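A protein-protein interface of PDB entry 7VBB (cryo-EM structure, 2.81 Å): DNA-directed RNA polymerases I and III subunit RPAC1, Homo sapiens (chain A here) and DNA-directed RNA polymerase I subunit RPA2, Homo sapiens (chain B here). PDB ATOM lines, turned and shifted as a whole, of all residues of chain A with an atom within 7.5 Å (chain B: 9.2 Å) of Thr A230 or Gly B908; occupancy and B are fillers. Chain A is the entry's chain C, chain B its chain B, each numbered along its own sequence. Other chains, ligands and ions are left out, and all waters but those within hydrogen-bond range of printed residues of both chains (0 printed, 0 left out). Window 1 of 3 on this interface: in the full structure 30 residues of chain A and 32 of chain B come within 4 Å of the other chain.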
ATOM      1  N   LEU A  61      23.660  -8.669  12.392  1.00  0.00           N
ATOM      2  CA  LEU A  61      24.763  -9.637  12.341  1.00  0.00           C
ATOM      3  C   LEU A  61      25.563  -9.255  13.570  1.00  0.00           C
ATOM      4  O   LEU A  61      25.466  -8.116  13.931  1.00  0.00           O
ATOM      5  CB  LEU A  61      25.545  -9.425  11.053  1.00  0.00           C
ATOM      6  CG  LEU A  61      26.568 -10.493  10.691  1.00  0.00           C
ATOM      7  CD1 LEU A  61      26.051 -11.877  11.020  1.00  0.00           C
ATOM      8  CD2 LEU A  61      26.927 -10.396   9.226  1.00  0.00           C
ATOM      9  N   ARG A  77      34.927  -1.101   9.496  1.00  0.00           N
ATOM     10  CA  ARG A  77      33.819  -0.314  10.033  1.00  0.00           C
ATOM     11  C   ARG A  77      33.580   0.947   9.211  1.00  0.00           C
ATOM     12  O   ARG A  77      32.432   1.288   8.904  1.00  0.00           O
ATOM     13  CB  ARG A  77      34.097   0.036  11.494  1.00  0.00           C
ATOM     14  CG  ARG A  77      33.003   0.819  12.172  1.00  0.00           C
ATOM     15  CD  ARG A  77      33.534   1.546  13.386  1.00  0.00           C
ATOM     16  NE  ARG A  77      34.430   2.635  13.018  1.00  0.00           N
ATOM     17  CZ  ARG A  77      34.059   3.904  12.909  1.00  0.00           C
ATOM     18  NH1 ARG A  77      32.804   4.250  13.139  1.00  0.00           N
ATOM     19  NH2 ARG A  77      34.943   4.828  12.570  1.00  0.00           N
ATOM     20  N   LEU A  80      31.776   0.192   5.754  1.00  0.00           N
ATOM     21  CA  LEU A  80      30.329  -0.054   5.793  1.00  0.00           C
ATOM     22  C   LEU A  80      29.590   1.273   5.942  1.00  0.00           C
ATOM     23  O   LEU A  80      28.672   1.512   5.162  1.00  0.00           O
ATOM     24  CB  LEU A  80      30.064  -1.048   6.920  1.00  0.00           C
ATOM     25  CG  LEU A  80      30.325  -2.505   6.576  1.00  0.00           C
ATOM     26  CD1 LEU A  80      30.727  -3.287   7.807  1.00  0.00           C
ATOM     27  CD2 LEU A  80      29.097  -3.114   5.939  1.00  0.00           C
ATOM     28  N   LEU A  81      30.020   2.144   6.839  1.00  0.00           N
ATOM     29  CA  LEU A  81      29.360   3.450   7.059  1.00  0.00           C
ATOM     30  C   LEU A  81      29.472   4.349   5.838  1.00  0.00           C
ATOM     31  O   LEU A  81      28.467   4.898   5.465  1.00  0.00           O
ATOM     32  CB  LEU A  81      29.960   4.147   8.281  1.00  0.00           C
ATOM     33  CG  LEU A  81      29.682   3.529   9.643  1.00  0.00           C
ATOM     34  CD1 LEU A  81      30.413   4.314  10.712  1.00  0.00           C
ATOM     35  CD2 LEU A  81      28.195   3.521   9.934  1.00  0.00           C
ATOM     36  N   SER A 226      23.932   5.887   2.603  1.00  0.00           N
ATOM     37  CA  SER A 226      24.630   4.963   3.525  1.00  0.00           C
ATOM     38  C   SER A 226      23.799   3.707   3.787  1.00  0.00           C
ATOM     39  O   SER A 226      22.636   3.881   4.151  1.00  0.00           O
ATOM     40  CB  SER A 226      25.004   5.620   4.787  1.00  0.00           C
ATOM     41  OG  SER A 226      25.685   4.724   5.642  1.00  0.00           O
ATOM     42  N   PRO A 227      24.324   2.457   3.706  1.00  0.00           N
ATOM     43  CA  PRO A 227      23.483   1.281   3.824  1.00  0.00           C
ATOM     44  C   PRO A 227      23.259   0.622   5.175  1.00  0.00           C
ATOM     45  O   PRO A 227      22.574  -0.338   5.171  1.00  0.00           O
ATOM     46  CB  PRO A 227      24.343   0.333   3.031  1.00  0.00           C
ATOM     47  CG  PRO A 227      25.737   0.642   3.474  1.00  0.00           C
ATOM     48  CD  PRO A 227      25.741   2.149   3.502  1.00  0.00           C
ATOM     49  N   VAL A 228      23.789   1.171   6.262  1.00  0.00           N
ATOM     50  CA  VAL A 228      23.732   0.547   7.608  1.00  0.00           C
ATOM     51  C   VAL A 228      23.276   1.564   8.642  1.00  0.00           C
ATOM     52  O   VAL A 228      23.638   2.712   8.474  1.00  0.00           O
ATOM     53  CB  VAL A 228      25.125   0.015   7.994  1.00  0.00           C
ATOM     54  CG1 VAL A 228      25.563  -1.186   7.184  1.00  0.00           C
ATOM     55  CG2 VAL A 228      26.195   1.085   7.983  1.00  0.00           C
ATOM     56  N   ALA A 229      22.431   1.183   9.602  1.00  0.00           N
ATOM     57  CA  ALA A 229      22.145   2.054  10.736  1.00  0.00           C
ATOM     58  C   ALA A 229      23.426   2.366  11.495  1.00  0.00           C
ATOM     59  O   ALA A 229      23.864   3.519  11.562  1.00  0.00           O
ATOM     60  CB  ALA A 229      21.115   1.405  11.657  1.00  0.00           C
ATOM     61  N   THR A 230      24.054   1.340  12.062  1.00  0.00           N
ATOM     62  CA  THR A 230      25.394   1.464  12.610  1.00  0.00           C
ATOM     63  C   THR A 230      26.157   0.179  12.333  1.00  0.00           C
ATOM     64  O   THR A 230      25.569  -0.896  12.216  1.00  0.00           O
ATOM     65  CB  THR A 230      25.381   1.750  14.114  1.00  0.00           C
ATOM     66  OG1 THR A 230      24.542   0.797  14.776  1.00  0.00           O
ATOM     67  CG2 THR A 230      24.872   3.152  14.382  1.00  0.00           C
ATOM     68  N   ALA A 231      27.478   0.308  12.229  1.00  0.00           N
ATOM     69  CA  ALA A 231      28.356  -0.817  11.946  1.00  0.00           C
ATOM     70  C   ALA A 231      29.518  -0.863  12.927  1.00  0.00           C
ATOM     71  O   ALA A 231      30.587  -1.387  12.608  1.00  0.00           O
ATOM     72  CB  ALA A 231      28.870  -0.757  10.510  1.00  0.00           C
ATOM     73  N   SER A 232      29.322  -0.328  14.127  1.00  0.00           N
ATOM     74  CA  SER A 232      30.411  -0.200  15.076  1.00  0.00           C
ATOM     75  C   SER A 232      30.902  -1.570  15.538  1.00  0.00           C
ATOM     76  O   SER A 232      30.345  -2.615  15.198  1.00  0.00           O
ATOM     77  CB  SER A 232      29.971   0.629  16.279  1.00  0.00           C
ATOM     78  OG  SER A 232      28.867   0.024  16.925  1.00  0.00           O
ATOM     79  N   TYR A 233      31.959  -1.574  16.344  1.00  0.00           N
ATOM     80  CA  TYR A 233      32.553  -2.779  16.955  1.00  0.00           C
ATOM     81  C   TYR A 233      33.007  -2.426  18.359  1.00  0.00           C
ATOM     82  O   TYR A 233      33.060  -1.264  18.669  1.00  0.00           O
ATOM     83  CB  TYR A 233      33.831  -3.179  16.240  1.00  0.00           C
ATOM     84  CG  TYR A 233      34.969  -2.204  16.135  1.00  0.00           C
ATOM     85  CD1 TYR A 233      35.752  -1.889  17.227  1.00  0.00           C
ATOM     86  CD2 TYR A 233      35.327  -1.688  14.907  1.00  0.00           C
ATOM     87  CE1 TYR A 233      36.813  -1.014  17.123  1.00  0.00           C
ATOM     88  CE2 TYR A 233      36.389  -0.816  14.783  1.00  0.00           C
ATOM     89  CZ  TYR A 233      37.130  -0.482  15.894  1.00  0.00           C
ATOM     90  OH  TYR A 233      38.178   0.369  15.775  1.00  0.00           O
ATOM     91  N   ARG A 234      33.232  -3.407  19.211  1.00  0.00           N
ATOM     92  CA  ARG A 234      33.731  -3.197  20.586  1.00  0.00           C
ATOM     93  C   ARG A 234      34.678  -4.336  20.931  1.00  0.00           C
ATOM     94  O   ARG A 234      34.396  -5.442  20.581  1.00  0.00           O
ATOM     95  CB  ARG A 234      32.568  -3.138  21.565  1.00  0.00           C
ATOM     96  CG  ARG A 234      31.953  -4.474  21.917  1.00  0.00           C
ATOM     97  CD  ARG A 234      30.603  -4.119  22.469  1.00  0.00           C
ATOM     98  NE  ARG A 234      29.976  -5.341  22.901  1.00  0.00           N
ATOM     99  CZ  ARG A 234      29.967  -5.738  24.151  1.00  0.00           C
ATOM    100  NH1 ARG A 234      29.377  -6.871  24.466  1.00  0.00           N
ATOM    101  NH2 ARG A 234      30.530  -4.998  25.085  1.00  0.00           N
ATOM    102  N   SER A 309      28.791  -5.471  14.913  1.00  0.00           N
ATOM    103  CA  SER A 309      27.333  -5.451  14.880  1.00  0.00           C
ATOM    104  C   SER A 309      26.914  -4.579  13.708  1.00  0.00           C
ATOM    105  O   SER A 309      27.037  -3.355  13.776  1.00  0.00           O
ATOM    106  CB  SER A 309      26.758  -4.917  16.184  1.00  0.00           C
ATOM    107  OG  SER A 309      26.654  -3.507  16.135  1.00  0.00           O
ATOM    108  N   VAL A 310      26.423  -5.203  12.645  1.00  0.00           N
ATOM    109  CA  VAL A 310      25.995  -4.501  11.443  1.00  0.00           C
ATOM    110  C   VAL A 310      24.482  -4.613  11.340  1.00  0.00           C
ATOM    111  O   VAL A 310      23.928  -5.713  11.444  1.00  0.00           O
ATOM    112  CB  VAL A 310      26.679  -5.068  10.189  1.00  0.00           C
ATOM    113  CG1 VAL A 310      26.203  -4.339   8.951  1.00  0.00           C
ATOM    114  CG2 VAL A 310      28.183  -4.974  10.326  1.00  0.00           C
ATOM    115  N   GLU A 311      23.817  -3.479  11.140  1.00  0.00           N
ATOM    116  CA  GLU A 311      22.364  -3.426  11.001  1.00  0.00           C
ATOM    117  C   GLU A 311      22.040  -2.639   9.742  1.00  0.00           C
ATOM    118  O   GLU A 311      22.227  -1.420   9.706  1.00  0.00           O
ATOM    119  CB  GLU A 311      21.712  -2.784  12.222  1.00  0.00           C
ATOM    120  CG  GLU A 311      22.249  -3.284  13.544  1.00  0.00           C
ATOM    121  CD  GLU A 311      22.075  -2.275  14.658  1.00  0.00           C
ATOM    122  OE1 GLU A 311      21.009  -1.627  14.715  1.00  0.00           O
ATOM    123  OE2 GLU A 311      23.006  -2.127  15.477  1.00  0.00           O
ATOM    124  N   SER A 312      21.555  -3.328   8.715  1.00  0.00           N
ATOM    125  CA  SER A 312      21.259  -2.656   7.464  1.00  0.00           C
ATOM    126  C   SER A 312      19.889  -1.994   7.522  1.00  0.00           C
ATOM    127  O   SER A 312      19.022  -2.360   8.319  1.00  0.00           O
ATOM    128  CB  SER A 312      21.316  -3.634   6.294  1.00  0.00           C
ATOM    129  OG  SER A 312      20.348  -4.654   6.444  1.00  0.00           O
ATOM    130  N   THR A 313      19.699  -1.001   6.657  1.00  0.00           N
ATOM    131  CA  THR A 313      18.401  -0.352   6.553  1.00  0.00           C
ATOM    132  C   THR A 313      17.377  -1.247   5.867  1.00  0.00           C
ATOM    133  O   THR A 313      16.182  -1.151   6.162  1.00  0.00           O
ATOM    134  CB  THR A 313      18.528   0.973   5.804  1.00  0.00           C
ATOM    135  OG1 THR A 313      19.258   0.768   4.590  1.00  0.00           O
ATOM    136  CG2 THR A 313      19.258   1.991   6.656  1.00  0.00           C
ATOM    137  N   ARG B 766      20.876  14.439   7.720  1.00  0.00           N
ATOM    138  CA  ARG B 766      19.619  13.789   8.053  1.00  0.00           C
ATOM    139  C   ARG B 766      18.584  14.760   8.598  1.00  0.00           C
ATOM    140  O   ARG B 766      17.584  14.323   9.173  1.00  0.00           O
ATOM    141  CB  ARG B 766      19.850  12.669   9.061  1.00  0.00           C
ATOM    142  CG  ARG B 766      20.427  11.407   8.475  1.00  0.00           C
ATOM    143  CD  ARG B 766      21.032  10.566   9.569  1.00  0.00           C
ATOM    144  NE  ARG B 766      21.897   9.521   9.047  1.00  0.00           N
ATOM    145  CZ  ARG B 766      23.026   9.141   9.628  1.00  0.00           C
ATOM    146  NH1 ARG B 766      23.430   9.728  10.741  1.00  0.00           N
ATOM    147  NH2 ARG B 766      23.757   8.179   9.086  1.00  0.00           N
ATOM    148  N   ALA B 899      30.879  11.471   9.456  1.00  0.00           N
ATOM    149  CA  ALA B 899      30.250  10.587  10.426  1.00  0.00           C
ATOM    150  C   ALA B 899      31.092   9.357  10.723  1.00  0.00           C
ATOM    151  O   ALA B 899      30.831   8.671  11.715  1.00  0.00           O
ATOM    152  CB  ALA B 899      28.868  10.161   9.935  1.00  0.00           C
ATOM    153  N   MET B 902      33.981  10.401  13.578  1.00  0.00           N
ATOM    154  CA  MET B 902      33.541  10.757  14.915  1.00  0.00           C
ATOM    155  C   MET B 902      33.841   9.622  15.888  1.00  0.00           C
ATOM    156  O   MET B 902      33.787   8.449  15.519  1.00  0.00           O
ATOM    157  CB  MET B 902      32.045  11.052  14.926  1.00  0.00           C
ATOM    158  CG  MET B 902      31.616  12.231  14.077  1.00  0.00           C
ATOM    159  SD  MET B 902      32.013  13.823  14.813  1.00  0.00           S
ATOM    160  CE  MET B 902      30.684  13.988  15.987  1.00  0.00           C
ATOM    161  N   PRO B 903      34.153   9.949  17.142  1.00  0.00           N
ATOM    162  CA  PRO B 903      34.437   8.901  18.130  1.00  0.00           C
ATOM    163  C   PRO B 903      33.163   8.161  18.506  1.00  0.00           C
ATOM    164  O   PRO B 903      32.260   8.729  19.121  1.00  0.00           O
ATOM    165  CB  PRO B 903      35.010   9.683  19.314  1.00  0.00           C
ATOM    166  CG  PRO B 903      34.407  11.026  19.195  1.00  0.00           C
ATOM    167  CD  PRO B 903      34.206  11.296  17.732  1.00  0.00           C
ATOM    168  N   PHE B 904      33.091   6.887  18.138  1.00  0.00           N
ATOM    169  CA  PHE B 904      31.917   6.086  18.437  1.00  0.00           C
ATOM    170  C   PHE B 904      32.032   5.483  19.827  1.00  0.00           C
ATOM    171  O   PHE B 904      33.122   5.157  20.297  1.00  0.00           O
ATOM    172  CB  PHE B 904      31.719   4.978  17.404  1.00  0.00           C
ATOM    173  CG  PHE B 904      32.922   4.103  17.204  1.00  0.00           C
ATOM    174  CD1 PHE B 904      34.026   4.563  16.518  1.00  0.00           C
ATOM    175  CD2 PHE B 904      32.937   2.811  17.686  1.00  0.00           C
ATOM    176  CE1 PHE B 904      35.120   3.757  16.327  1.00  0.00           C
ATOM    177  CE2 PHE B 904      34.029   2.006  17.495  1.00  0.00           C
ATOM    178  CZ  PHE B 904      35.121   2.481  16.818  1.00  0.00           C
ATOM    179  N   THR B 905      30.891   5.333  20.480  1.00  0.00           N
ATOM    180  CA  THR B 905      30.833   4.809  21.831  1.00  0.00           C
ATOM    181  C   THR B 905      30.734   3.288  21.796  1.00  0.00           C
ATOM    182  O   THR B 905      30.541   2.671  20.749  1.00  0.00           O
ATOM    183  CB  THR B 905      29.662   5.432  22.591  1.00  0.00           C
ATOM    184  OG1 THR B 905      29.669   4.974  23.946  1.00  0.00           O
ATOM    185  CG2 THR B 905      28.354   5.060  21.942  1.00  0.00           C
ATOM    186  N   GLU B 906      30.873   2.675  22.971  1.00  0.00           N
ATOM    187  CA  GLU B 906      30.829   1.219  23.048  1.00  0.00           C
ATOM    188  C   GLU B 906      29.424   0.685  22.818  1.00  0.00           C
ATOM    189  O   GLU B 906      29.227  -0.532  22.752  1.00  0.00           O
ATOM    190  CB  GLU B 906      31.360   0.750  24.399  1.00  0.00           C
ATOM    191  CG  GLU B 906      31.755  -0.708  24.425  1.00  0.00           C
ATOM    192  CD  GLU B 906      32.110  -1.184  25.814  1.00  0.00           C
ATOM    193  OE1 GLU B 906      31.905  -0.414  26.776  1.00  0.00           O
ATOM    194  OE2 GLU B 906      32.594  -2.328  25.946  1.00  0.00           O
ATOM    195  N   SER B 907      28.438   1.571  22.707  1.00  0.00           N
ATOM    196  CA  SER B 907      27.063   1.183  22.421  1.00  0.00           C
ATOM    197  C   SER B 907      26.702   1.338  20.953  1.00  0.00           C
ATOM    198  O   SER B 907      25.544   1.118  20.590  1.00  0.00           O
ATOM    199  CB  SER B 907      26.103   2.010  23.274  1.00  0.00           C
ATOM    200  OG  SER B 907      26.332   1.795  24.653  1.00  0.00           O
ATOM    201  N   GLY B 908      27.658   1.703  20.104  1.00  0.00           N
ATOM    202  CA  GLY B 908      27.403   1.935  18.702  1.00  0.00           C
ATOM    203  C   GLY B 908      27.063   3.365  18.355  1.00  0.00           C
ATOM    204  O   GLY B 908      27.144   3.736  17.178  1.00  0.00           O
ATOM    205  N   MET B 909      26.691   4.176  19.340  1.00  0.00           N
ATOM    206  CA  MET B 909      26.264   5.536  19.076  1.00  0.00           C
ATOM    207  C   MET B 909      27.427   6.373  18.557  1.00  0.00           C
ATOM    208  O   MET B 909      28.580   5.943  18.526  1.00  0.00           O
ATOM    209  CB  MET B 909      25.691   6.172  20.340  1.00  0.00           C
ATOM    210  CG  MET B 909      24.379   5.576  20.810  1.00  0.00           C
ATOM    211  SD  MET B 909      23.602   6.654  22.013  1.00  0.00           S
ATOM    212  CE  MET B 909      23.930   8.236  21.249  1.00  0.00           C
ATOM    213  N   VAL B 910      27.108   7.598  18.158  1.00  0.00           N
ATOM    214  CA  VAL B 910      28.098   8.549  17.669  1.00  0.00           C
ATOM    215  C   VAL B 910      27.544   9.946  17.915  1.00  0.00           C
ATOM    216  O   VAL B 910      26.472  10.280  17.396  1.00  0.00           O
ATOM    217  CB  VAL B 910      28.407   8.325  16.181  1.00  0.00           C
ATOM    218  CG1 VAL B 910      29.145   9.515  15.614  1.00  0.00           C
ATOM    219  CG2 VAL B 910      29.225   7.070  15.994  1.00  0.00           C
ATOM    220  N   PRO B 911      28.223  10.790  18.686  1.00  0.00           N
ATOM    221  CA  PRO B 911      27.683  12.121  18.961  1.00  0.00           C
ATOM    222  C   PRO B 911      27.376  12.866  17.674  1.00  0.00           C
ATOM    223  O   PRO B 911      27.895  12.557  16.602  1.00  0.00           O
ATOM    224  CB  PRO B 911      28.807  12.806  19.746  1.00  0.00           C
ATOM    225  CG  PRO B 911      30.027  12.014  19.431  1.00  0.00           C
ATOM    226  CD  PRO B 911      29.553  10.610  19.285  1.00  0.00           C
ATOM    227  N   TYR B 971      24.104   2.374  32.724  1.00  0.00           N
ATOM    228  CA  TYR B 971      25.195   3.300  32.476  1.00  0.00           C
ATOM    229  C   TYR B 971      25.894   3.570  33.805  1.00  0.00           C
ATOM    230  O   TYR B 971      25.599   2.933  34.817  1.00  0.00           O
ATOM    231  CB  TYR B 971      24.662   4.553  31.790  1.00  0.00           C
ATOM    232  CG  TYR B 971      24.326   4.316  30.339  1.00  0.00           C
ATOM    233  CD1 TYR B 971      23.241   3.533  29.977  1.00  0.00           C
ATOM    234  CD2 TYR B 971      25.106   4.854  29.330  1.00  0.00           C
ATOM    235  CE1 TYR B 971      22.938   3.303  28.656  1.00  0.00           C
ATOM    236  CE2 TYR B 971      24.808   4.630  28.002  1.00  0.00           C
ATOM    237  CZ  TYR B 971      23.726   3.854  27.672  1.00  0.00           C
ATOM    238  OH  TYR B 971      23.428   3.632  26.349  1.00  0.00           O
ATOM    239  N   GLU B 977      30.680   7.619  29.440  1.00  0.00           N
ATOM    240  CA  GLU B 977      30.795   6.392  28.672  1.00  0.00           C
ATOM    241  C   GLU B 977      32.067   6.473  27.845  1.00  0.00           C
ATOM    242  O   GLU B 977      32.447   7.549  27.378  1.00  0.00           O
ATOM    243  CB  GLU B 977      29.579   6.187  27.764  1.00  0.00           C
ATOM    244  CG  GLU B 977      29.633   4.937  26.893  1.00  0.00           C
ATOM    245  CD  GLU B 977      29.521   3.646  27.689  1.00  0.00           C
ATOM    246  OE1 GLU B 977      28.901   3.659  28.774  1.00  0.00           O
ATOM    247  OE2 GLU B 977      30.051   2.615  27.227  1.00  0.00           O
ATOM    248  N   ARG B 978      32.726   5.337  27.659  1.00  0.00           N
ATOM    249  CA  ARG B 978      34.027   5.335  27.009  1.00  0.00           C
ATOM    250  C   ARG B 978      33.896   5.102  25.513  1.00  0.00           C
ATOM    251  O   ARG B 978      33.229   4.166  25.067  1.00  0.00           O
ATOM    252  CB  ARG B 978      34.949   4.287  27.627  1.00  0.00           C
ATOM    253  CG  ARG B 978      34.395   2.897  27.711  1.00  0.00           C
ATOM    254  CD  ARG B 978      35.396   2.033  28.437  1.00  0.00           C
ATOM    255  NE  ARG B 978      35.987   2.753  29.561  1.00  0.00           N
ATOM    256  CZ  ARG B 978      37.190   3.319  29.543  1.00  0.00           C
ATOM    257  NH1 ARG B 978      37.943   3.259  28.454  1.00  0.00           N
ATOM    258  NH2 ARG B 978      37.639   3.957  30.615  1.00  0.00           N
ATOM    259  N   LEU B 979      34.555   5.961  24.749  1.00  0.00           N
ATOM    260  CA  LEU B 979      34.457   6.011  23.303  1.00  0.00           C
ATOM    261  C   LEU B 979      35.667   5.343  22.667  1.00  0.00           C
ATOM    262  O   LEU B 979      36.658   5.032  23.328  1.00  0.00           O
ATOM    263  CB  LEU B 979      34.351   7.464  22.827  1.00  0.00           C
ATOM    264  CG  LEU B 979      32.984   8.141  22.863  1.00  0.00           C
ATOM    265  CD1 LEU B 979      32.400   8.104  24.255  1.00  0.00           C
ATOM    266  CD2 LEU B 979      33.110   9.564  22.381  1.00  0.00           C
ATOM    267  N   TYR B 980      35.564   5.118  21.363  1.00  0.00           N
ATOM    268  CA  TYR B 980      36.688   4.739  20.527  1.00  0.00           C
ATOM    269  C   TYR B 980      37.025   5.896  19.600  1.00  0.00           C
ATOM    270  O   TYR B 980      36.214   6.796  19.381  1.00  0.00           O
ATOM    271  CB  TYR B 980      36.381   3.486  19.699  1.00  0.00           C
ATOM    272  CG  TYR B 980      36.225   2.229  20.511  1.00  0.00           C
ATOM    273  CD1 TYR B 980      35.140   2.054  21.349  1.00  0.00           C
ATOM    274  CD2 TYR B 980      37.164   1.213  20.436  1.00  0.00           C
ATOM    275  CE1 TYR B 980      34.993   0.911  22.092  1.00  0.00           C
ATOM    276  CE2 TYR B 980      37.027   0.068  21.175  1.00  0.00           C
ATOM    277  CZ  TYR B 980      35.939  -0.078  22.003  1.00  0.00           C
ATOM    278  OH  TYR B 980      35.792  -1.222  22.747  1.00  0.00           O
ATOM    279  N   ILE B 994      29.236  12.106  27.922  1.00  0.00           N
ATOM    280  CA  ILE B 994      28.291  12.258  26.825  1.00  0.00           C
ATOM    281  C   ILE B 994      26.877  12.283  27.387  1.00  0.00           C
ATOM    282  O   ILE B 994      26.606  11.742  28.463  1.00  0.00           O
ATOM    283  CB  ILE B 994      28.461  11.139  25.773  1.00  0.00           C
ATOM    284  CG1 ILE B 994      27.641  11.457  24.523  1.00  0.00           C
ATOM    285  CG2 ILE B 994      28.096   9.792  26.361  1.00  0.00           C
ATOM    286  CD1 ILE B 994      28.019  10.648  23.315  1.00  0.00           C
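OE2 of Glu B906 is in salt-bridge range of NH2 of Arg A234 (3.5 Å).
Among the printed residues, merely in contact across the chains: Ser A232 with Gly B908 (3.0 Å), Arg A77 with Phe B904 (3.6 Å), Arg A234 with Tyr B980 (3.6 Å), Tyr A233 with Phe B904 (3.6 Å), Thr A230 with Gly B908 (3.6 Å) and Ser A232 with Phe B904 (3.9 Å).
Val A228 touches none of the printed residues of chain B.
No residue of chain B comes within 4 Å of Ala A229.
Of the printed residues of chain B, Thr A230 touches Gly B908.
No residue of chain B comes within 4 Å of Ala A231.
Printed residues of chain B within 4 Å of Tyr A233: Phe B904.
Of the printed residues of chain A, Phe B904 touches Arg A77 (3.6 Å), Ser A232 (3.9 Å) and Tyr A233 (3.6 Å).
Ser B907 touches none of the printed residues of chain A.
Of chain A, only Thr A230 and Ser A232 come within 4 Å of Gly B908.
The nearest residue of chain B that does not touch Thr A230 is Met B909 (5.4 Å).
O of Phe B904 lies within hydrogen-bond range of N of Tyr B980 (2.7 Å).
The backbone carbonyl oxygen of Arg B978 is in hydrogen-bond range of the backbone NH of Glu B906, 3.5 Å away.
O of Thr A230 lies within hydrogen-bond range of N of Glu A311 (3.3 Å).
The backbone carbonyl oxygen (O) of Ser A232 is in hydrogen-bond range of the backbone NH (N) of Ser A309 (3.3 Å).
Of the 18 printed residues of chain A, 5 touch a printed residue of chain B.
Hydrophobic or aromatic side chains of chain A that line the printed part of chain B: Tyr A233.
Of the 18 printed residues of chain B, 4 touch a printed residue of chain A.
Hydrophobic or aromatic side chains of chain B that line the printed part of chain A: Phe B904 and Tyr B980.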
